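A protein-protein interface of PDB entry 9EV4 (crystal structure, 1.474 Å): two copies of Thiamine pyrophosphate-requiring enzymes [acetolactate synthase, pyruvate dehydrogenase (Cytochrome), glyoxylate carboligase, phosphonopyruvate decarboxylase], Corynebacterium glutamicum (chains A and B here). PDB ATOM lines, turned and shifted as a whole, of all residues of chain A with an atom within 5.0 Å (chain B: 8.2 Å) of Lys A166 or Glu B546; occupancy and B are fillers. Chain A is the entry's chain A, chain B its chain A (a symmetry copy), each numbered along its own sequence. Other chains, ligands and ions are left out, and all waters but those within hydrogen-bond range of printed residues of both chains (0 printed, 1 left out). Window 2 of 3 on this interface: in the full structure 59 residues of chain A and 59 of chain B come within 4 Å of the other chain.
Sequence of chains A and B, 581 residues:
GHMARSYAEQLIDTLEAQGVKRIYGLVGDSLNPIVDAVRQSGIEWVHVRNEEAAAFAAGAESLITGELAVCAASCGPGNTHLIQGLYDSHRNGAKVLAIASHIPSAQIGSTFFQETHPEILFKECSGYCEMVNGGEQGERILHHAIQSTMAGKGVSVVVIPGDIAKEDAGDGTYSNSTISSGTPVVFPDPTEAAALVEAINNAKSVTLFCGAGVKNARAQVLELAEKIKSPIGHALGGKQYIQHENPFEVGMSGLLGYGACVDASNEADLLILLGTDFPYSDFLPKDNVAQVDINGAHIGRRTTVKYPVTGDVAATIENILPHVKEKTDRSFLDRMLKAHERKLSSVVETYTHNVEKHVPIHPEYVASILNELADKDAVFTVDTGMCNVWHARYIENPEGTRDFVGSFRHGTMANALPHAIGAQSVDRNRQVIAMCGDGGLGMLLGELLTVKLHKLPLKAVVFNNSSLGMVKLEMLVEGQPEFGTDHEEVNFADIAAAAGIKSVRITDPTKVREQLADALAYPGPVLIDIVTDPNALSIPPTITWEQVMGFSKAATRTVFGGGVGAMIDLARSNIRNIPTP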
ATOM      1  N   SER A   6     -18.114   4.496   5.260  1.00  0.00           N
ATOM      2  CA  SER A   6     -18.360   3.202   4.644  1.00  0.00           C
ATOM      3  C   SER A   6     -19.852   2.833   4.575  1.00  0.00           C
ATOM      4  O   SER A   6     -20.680   3.422   5.273  1.00  0.00           O
ATOM      5  CB  SER A   6     -17.637   2.129   5.453  1.00  0.00           C
ATOM      6  OG  SER A   6     -18.283   1.918   6.702  1.00  0.00           O
ATOM      7  N   PRO A  33     -16.977  -5.324  10.280  1.00  0.00           N
ATOM      8  CA  PRO A  33     -17.176  -3.894   9.991  1.00  0.00           C
ATOM      9  C   PRO A  33     -18.540  -3.398  10.484  1.00  0.00           C
ATOM     10  O   PRO A  33     -18.645  -2.244  10.928  1.00  0.00           O
ATOM     11  CB  PRO A  33     -17.068  -3.807   8.458  1.00  0.00           C
ATOM     12  CG  PRO A  33     -16.362  -5.052   8.042  1.00  0.00           C
ATOM     13  CD  PRO A  33     -16.741  -6.102   9.048  1.00  0.00           C
ATOM     14  N   GLY A 162     -19.039  -9.609   2.628  1.00  0.00           N
ATOM     15  CA  GLY A 162     -18.269  -8.993   3.707  1.00  0.00           C
ATOM     16  C   GLY A 162     -17.405  -7.799   3.334  1.00  0.00           C
ATOM     17  O   GLY A 162     -17.393  -6.784   4.045  1.00  0.00           O
ATOM     18  N   ASP A 163     -16.681  -7.901   2.213  1.00  0.00           N
ATOM     19  CA  ASP A 163     -15.803  -6.825   1.736  1.00  0.00           C
ATOM     20  C   ASP A 163     -16.559  -5.525   1.371  1.00  0.00           C
ATOM     21  O   ASP A 163     -16.019  -4.438   1.551  1.00  0.00           O
ATOM     22  CB  ASP A 163     -15.025  -7.299   0.490  1.00  0.00           C
ATOM     23  CG  ASP A 163     -15.885  -7.780  -0.674  1.00  0.00           C
ATOM     24  OD1 ASP A 163     -16.904  -8.484  -0.422  1.00  0.00           O
ATOM     25  OD2 ASP A 163     -15.515  -7.503  -1.843  1.00  0.00           O
ATOM     26  N   ILE A 164     -17.796  -5.628   0.841  1.00  0.00           N
ATOM     27  CA  ILE A 164     -18.549  -4.439   0.423  1.00  0.00           C
ATOM     28  C   ILE A 164     -18.968  -3.584   1.603  1.00  0.00           C
ATOM     29  O   ILE A 164     -19.072  -2.371   1.438  1.00  0.00           O
ATOM     30  CB  ILE A 164     -19.769  -4.811  -0.457  1.00  0.00           C
ATOM     31  CG1 ILE A 164     -19.260  -5.590  -1.677  1.00  0.00           C
ATOM     32  CG2 ILE A 164     -20.538  -3.524  -0.897  1.00  0.00           C
ATOM     33  CD1 ILE A 164     -20.351  -6.097  -2.550  1.00  0.00           C
ATOM     34  N   ALA A 165     -19.097  -4.163   2.829  1.00  0.00           N
ATOM     35  CA  ALA A 165     -19.370  -3.328   4.006  1.00  0.00           C
ATOM     36  C   ALA A 165     -18.266  -2.256   4.204  1.00  0.00           C
ATOM     37  O   ALA A 165     -18.540  -1.186   4.749  1.00  0.00           O
ATOM     38  CB  ALA A 165     -19.467  -4.192   5.253  1.00  0.00           C
ATOM     39  N   LYS A 166     -17.017  -2.542   3.758  1.00  0.00           N
ATOM     40  CA  LYS A 166     -15.927  -1.564   3.918  1.00  0.00           C
ATOM     41  C   LYS A 166     -15.814  -0.556   2.759  1.00  0.00           C
ATOM     42  O   LYS A 166     -15.085   0.438   2.877  1.00  0.00           O
ATOM     43  CB  LYS A 166     -14.585  -2.275   4.120  1.00  0.00           C
ATOM     44  CG  LYS A 166     -14.574  -3.123   5.393  1.00  0.00           C
ATOM     45  CD  LYS A 166     -13.155  -3.496   5.854  1.00  0.00           C
ATOM     46  CE  LYS A 166     -12.261  -2.311   6.156  1.00  0.00           C
ATOM     47  NZ  LYS A 166     -10.882  -2.751   6.525  1.00  0.00           N
ATOM     48  N   GLU A 167     -16.540  -0.773   1.661  1.00  0.00           N
ATOM     49  CA  GLU A 167     -16.542   0.184   0.537  1.00  0.00           C
ATOM     50  C   GLU A 167     -17.301   1.484   0.913  1.00  0.00           C
ATOM     51  O   GLU A 167     -18.099   1.502   1.850  1.00  0.00           O
ATOM     52  CB  GLU A 167     -17.217  -0.435  -0.708  1.00  0.00           C
ATOM     53  CG  GLU A 167     -16.502  -1.624  -1.335  1.00  0.00           C
ATOM     54  CD  GLU A 167     -17.196  -2.161  -2.583  1.00  0.00           C
ATOM     55  OE1 GLU A 167     -16.788  -3.245  -3.062  1.00  0.00           O
ATOM     56  OE2 GLU A 167     -18.134  -1.502  -3.093  1.00  0.00           O
ATOM     57  N   ASP A 168     -17.110   2.536   0.135  1.00  0.00           N
ATOM     58  CA  ASP A 168     -17.757   3.818   0.390  1.00  0.00           C
ATOM     59  C   ASP A 168     -19.282   3.708   0.383  1.00  0.00           C
ATOM     60  O   ASP A 168     -19.867   2.964  -0.414  1.00  0.00           O
ATOM     61  CB  ASP A 168     -17.331   4.872  -0.652  1.00  0.00           C
ATOM     62  CG  ASP A 168     -15.896   5.344  -0.540  1.00  0.00           C
ATOM     63  OD1 ASP A 168     -15.267   5.099   0.508  1.00  0.00           O
ATOM     64  OD2 ASP A 168     -15.399   5.948  -1.505  1.00  0.00           O
ATOM     65  N   LEU B 255      -3.513 -20.014   6.981  1.00  0.00           N
ATOM     66  CA  LEU B 255      -3.284 -19.356   8.285  1.00  0.00           C
ATOM     67  C   LEU B 255      -3.065 -20.366   9.438  1.00  0.00           C
ATOM     68  O   LEU B 255      -2.361 -20.052  10.406  1.00  0.00           O
ATOM     69  CB  LEU B 255      -4.443 -18.414   8.636  1.00  0.00           C
ATOM     70  CG  LEU B 255      -4.488 -17.095   7.807  1.00  0.00           C
ATOM     71  CD1 LEU B 255      -5.756 -16.285   8.134  1.00  0.00           C
ATOM     72  CD2 LEU B 255      -3.263 -16.224   8.107  1.00  0.00           C
ATOM     73  N   ASP B 282      -3.755 -16.807  -1.980  1.00  0.00           N
ATOM     74  CA  ASP B 282      -2.615 -15.943  -1.657  1.00  0.00           C
ATOM     75  C   ASP B 282      -1.384 -16.738  -1.150  1.00  0.00           C
ATOM     76  O   ASP B 282      -0.287 -16.187  -1.101  1.00  0.00           O
ATOM     77  CB  ASP B 282      -2.995 -14.815  -0.683  1.00  0.00           C
ATOM     78  CG  ASP B 282      -3.679 -15.224   0.614  1.00  0.00           C
ATOM     79  OD1 ASP B 282      -4.235 -16.337   0.668  1.00  0.00           O
ATOM     80  OD2 ASP B 282      -3.706 -14.396   1.564  1.00  0.00           O
ATOM     81  N   THR B 542       0.717  -8.078  11.447  1.00  0.00           N
ATOM     82  CA  THR B 542       0.599  -7.937   9.998  1.00  0.00           C
ATOM     83  C   THR B 542      -0.642  -8.681   9.447  1.00  0.00           C
ATOM     84  O   THR B 542      -1.044  -8.379   8.327  1.00  0.00           O
ATOM     85  CB  THR B 542       1.876  -8.413   9.302  1.00  0.00           C
ATOM     86  OG1 THR B 542       2.146  -9.758   9.703  1.00  0.00           O
ATOM     87  CG2 THR B 542       3.077  -7.514   9.608  1.00  0.00           C
ATOM     88  N   ILE B 543      -1.244  -9.630  10.200  1.00  0.00           N
ATOM     89  CA  ILE B 543      -2.444 -10.332   9.689  1.00  0.00           C
ATOM     90  C   ILE B 543      -3.660  -9.392   9.704  1.00  0.00           C
ATOM     91  O   ILE B 543      -4.107  -8.956  10.767  1.00  0.00           O
ATOM     92  CB  ILE B 543      -2.751 -11.670  10.411  1.00  0.00           C
ATOM     93  CG1 ILE B 543      -1.631 -12.697  10.126  1.00  0.00           C
ATOM     94  CG2 ILE B 543      -4.124 -12.226   9.977  1.00  0.00           C
ATOM     95  CD1 ILE B 543      -1.800 -14.048  10.745  1.00  0.00           C
ATOM     96  N   THR B 544      -4.197  -9.090   8.513  1.00  0.00           N
ATOM     97  CA  THR B 544      -5.332  -8.186   8.370  1.00  0.00           C
ATOM     98  C   THR B 544      -6.678  -8.935   8.368  1.00  0.00           C
ATOM     99  O   THR B 544      -6.712 -10.155   8.196  1.00  0.00           O
ATOM    100  CB  THR B 544      -5.169  -7.403   7.049  1.00  0.00           C
ATOM    101  OG1 THR B 544      -5.353  -8.311   5.951  1.00  0.00           O
ATOM    102  CG2 THR B 544      -3.819  -6.670   6.958  1.00  0.00           C
ATOM    103  N   TRP B 545      -7.787  -8.184   8.499  1.00  0.00           N
ATOM    104  CA  TRP B 545      -9.138  -8.719   8.403  1.00  0.00           C
ATOM    105  C   TRP B 545      -9.364  -9.282   6.976  1.00  0.00           C
ATOM    106  O   TRP B 545     -10.023 -10.302   6.827  1.00  0.00           O
ATOM    107  CB  TRP B 545     -10.169  -7.624   8.740  1.00  0.00           C
ATOM    108  CG  TRP B 545     -11.590  -8.097   8.656  1.00  0.00           C
ATOM    109  CD1 TRP B 545     -12.246  -8.889   9.549  1.00  0.00           C
ATOM    110  CD2 TRP B 545     -12.530  -7.799   7.612  1.00  0.00           C
ATOM    111  NE1 TRP B 545     -13.522  -9.148   9.104  1.00  0.00           N
ATOM    112  CE2 TRP B 545     -13.735  -8.460   7.933  1.00  0.00           C
ATOM    113  CE3 TRP B 545     -12.469  -7.037   6.438  1.00  0.00           C
ATOM    114  CZ2 TRP B 545     -14.854  -8.408   7.110  1.00  0.00           C
ATOM    115  CZ3 TRP B 545     -13.586  -6.985   5.624  1.00  0.00           C
ATOM    116  CH2 TRP B 545     -14.758  -7.669   5.962  1.00  0.00           C
ATOM    117  N   GLU B 546      -8.781  -8.649   5.942  1.00  0.00           N
ATOM    118  CA  GLU B 546      -8.891  -9.132   4.555  1.00  0.00           C
ATOM    119  C   GLU B 546      -8.294 -10.542   4.425  1.00  0.00           C
ATOM    120  O   GLU B 546      -8.842 -11.395   3.730  1.00  0.00           O
ATOM    121  CB  GLU B 546      -8.164  -8.170   3.594  1.00  0.00           C
ATOM    122  CG  GLU B 546      -8.880  -6.842   3.385  1.00  0.00           C
ATOM    123  CD  GLU B 546      -8.777  -5.840   4.521  1.00  0.00           C
ATOM    124  OE1 GLU B 546      -7.837  -5.967   5.342  1.00  0.00           O
ATOM    125  OE2 GLU B 546      -9.650  -4.943   4.607  1.00  0.00           O
ATOM    126  N   GLN B 547      -7.165 -10.780   5.107  1.00  0.00           N
ATOM    127  CA  GLN B 547      -6.468 -12.059   5.094  1.00  0.00           C
ATOM    128  C   GLN B 547      -7.261 -13.091   5.853  1.00  0.00           C
ATOM    129  O   GLN B 547      -7.420 -14.212   5.361  1.00  0.00           O
ATOM    130  CB  GLN B 547      -5.050 -11.914   5.687  1.00  0.00           C
ATOM    131  CG  GLN B 547      -4.083 -11.284   4.682  1.00  0.00           C
ATOM    132  CD  GLN B 547      -2.715 -11.022   5.268  1.00  0.00           C
ATOM    133  OE1 GLN B 547      -2.570 -10.778   6.464  1.00  0.00           O
ATOM    134  NE2 GLN B 547      -1.680 -11.040   4.428  1.00  0.00           N
ATOM    135  N   VAL B 548      -7.816 -12.717   7.026  1.00  0.00           N
ATOM    136  CA  VAL B 548      -8.671 -13.613   7.823  1.00  0.00           C
ATOM    137  C   VAL B 548      -9.892 -14.032   6.968  1.00  0.00           C
ATOM    138  O   VAL B 548     -10.240 -15.206   6.907  1.00  0.00           O
ATOM    139  CB  VAL B 548      -9.110 -12.903   9.140  1.00  0.00           C
ATOM    140  CG1 VAL B 548     -10.317 -13.593   9.787  1.00  0.00           C
ATOM    141  CG2 VAL B 548      -7.947 -12.819  10.124  1.00  0.00           C
ATOM    142  N   MET B 549     -10.477 -13.074   6.256  1.00  0.00           N
ATOM    143  CA  MET B 549     -11.654 -13.337   5.425  1.00  0.00           C
ATOM    144  C   MET B 549     -11.352 -14.022   4.076  1.00  0.00           C
ATOM    145  O   MET B 549     -12.277 -14.488   3.407  1.00  0.00           O
ATOM    146  CB  MET B 549     -12.427 -12.044   5.170  1.00  0.00           C
ATOM    147  CG  MET B 549     -13.161 -11.526   6.387  1.00  0.00           C
ATOM    148  SD  MET B 549     -14.228 -12.726   7.240  1.00  0.00           S
ATOM    149  CE  MET B 549     -15.244 -13.404   5.827  1.00  0.00           C
ATOM    150  N   GLY B 550     -10.090 -14.058   3.681  1.00  0.00           N
ATOM    151  CA  GLY B 550      -9.691 -14.735   2.459  1.00  0.00           C
ATOM    152  C   GLY B 550      -9.878 -13.957   1.178  1.00  0.00           C
ATOM    153  O   GLY B 550     -10.060 -14.580   0.126  1.00  0.00           O
ATOM    154  N   PHE B 551      -9.809 -12.604   1.226  1.00  0.00           N
ATOM    155  CA  PHE B 551      -9.892 -11.822  -0.014  1.00  0.00           C
ATOM    156  C   PHE B 551      -8.652 -10.894  -0.192  1.00  0.00           C
ATOM    157  O   PHE B 551      -8.671 -10.016  -1.050  1.00  0.00           O
ATOM    158  CB  PHE B 551     -11.224 -11.040  -0.180  1.00  0.00           C
ATOM    159  CG  PHE B 551     -11.510  -9.867   0.735  1.00  0.00           C
ATOM    160  CD1 PHE B 551     -12.082 -10.063   1.985  1.00  0.00           C
ATOM    161  CD2 PHE B 551     -11.293  -8.568   0.311  1.00  0.00           C
ATOM    162  CE1 PHE B 551     -12.417  -8.982   2.792  1.00  0.00           C
ATOM    163  CE2 PHE B 551     -11.562  -7.489   1.150  1.00  0.00           C
ATOM    164  CZ  PHE B 551     -12.120  -7.703   2.386  1.00  0.00           C
ATOM    165  N   SER B 552      -7.555 -11.125   0.566  1.00  0.00           N
ATOM    166  CA  SER B 552      -6.340 -10.322   0.391  1.00  0.00           C
ATOM    167  C   SER B 552      -5.549 -10.897  -0.781  1.00  0.00           C
ATOM    168  O   SER B 552      -5.295 -12.107  -0.821  1.00  0.00           O
ATOM    169  CB  SER B 552      -5.512 -10.314   1.670  1.00  0.00           C
ATOM    170  OG  SER B 552      -4.249  -9.694   1.466  1.00  0.00           O
ATOM    171  N   LYS B 553      -5.166 -10.040  -1.737  1.00  0.00           N
ATOM    172  CA  LYS B 553      -4.495 -10.476  -2.958  1.00  0.00           C
ATOM    173  C   LYS B 553      -2.996 -10.703  -2.814  1.00  0.00           C
ATOM    174  O   LYS B 553      -2.469 -11.618  -3.446  1.00  0.00           O
ATOM    175  CB  LYS B 553      -4.724  -9.449  -4.087  1.00  0.00           C
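CZ2 of Trp B545 touches CD of Pro A33 (3.6 Å).
Trp B545 touches Gly A162 (CH2 to O, 3.4 Å).
Phe B551 touches Asp A163.
Lys A166 touches Trp B545.
No position is printed for both chains.
Printed residues of chain B within 4 Å of Gly A162: Trp B545 (3.4 Å).
Lys A166 touches just these residues of chain B: Trp B545 and Glu B546.
Asp A168 touches none of the printed residues of chain B.
Glu B546 touches just one residue of chain A: Lys A166.
Of the printed residues of chain A, Phe B551 touches Asp A163 (3.5 Å).
The nearest printed residue of chain B that does not touch Asp A163 is Trp B545 (4.2 Å).
The side-chain amino group (NZ) of Lys A166 lies within salt-bridge range of the side-chain carboxylate (OE2) of Glu B546 (3.2 Å).
The backbone carbonyl oxygen (O) of Glu B546 is in hydrogen-bond range of the backbone NH (N) of Phe B551, at 2.9 Å.
The side-chain hydroxyl of Thr B544 lies close to the backbone NH of Glu B546 (3.4 Å).
N of Ser B552 is in hydrogen-bond range of O of Glu B546 (3.4 Å).
Hydrophobic or aromatic side chains of chain B within 4 Å of the printed part of chain A: Trp B545 and Phe B551.
Along chain B the printed residues that touch a printed residue of chain A span positions 545 to 551.
Among the printed residues, 5 pairs touch across the chains.
Among the printed residues, Asp or Glu carboxylates within 4 Å of a Lys or Arg side-chain nitrogen of the other chain: Lys A166 with Glu B546 (3.2 Å).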
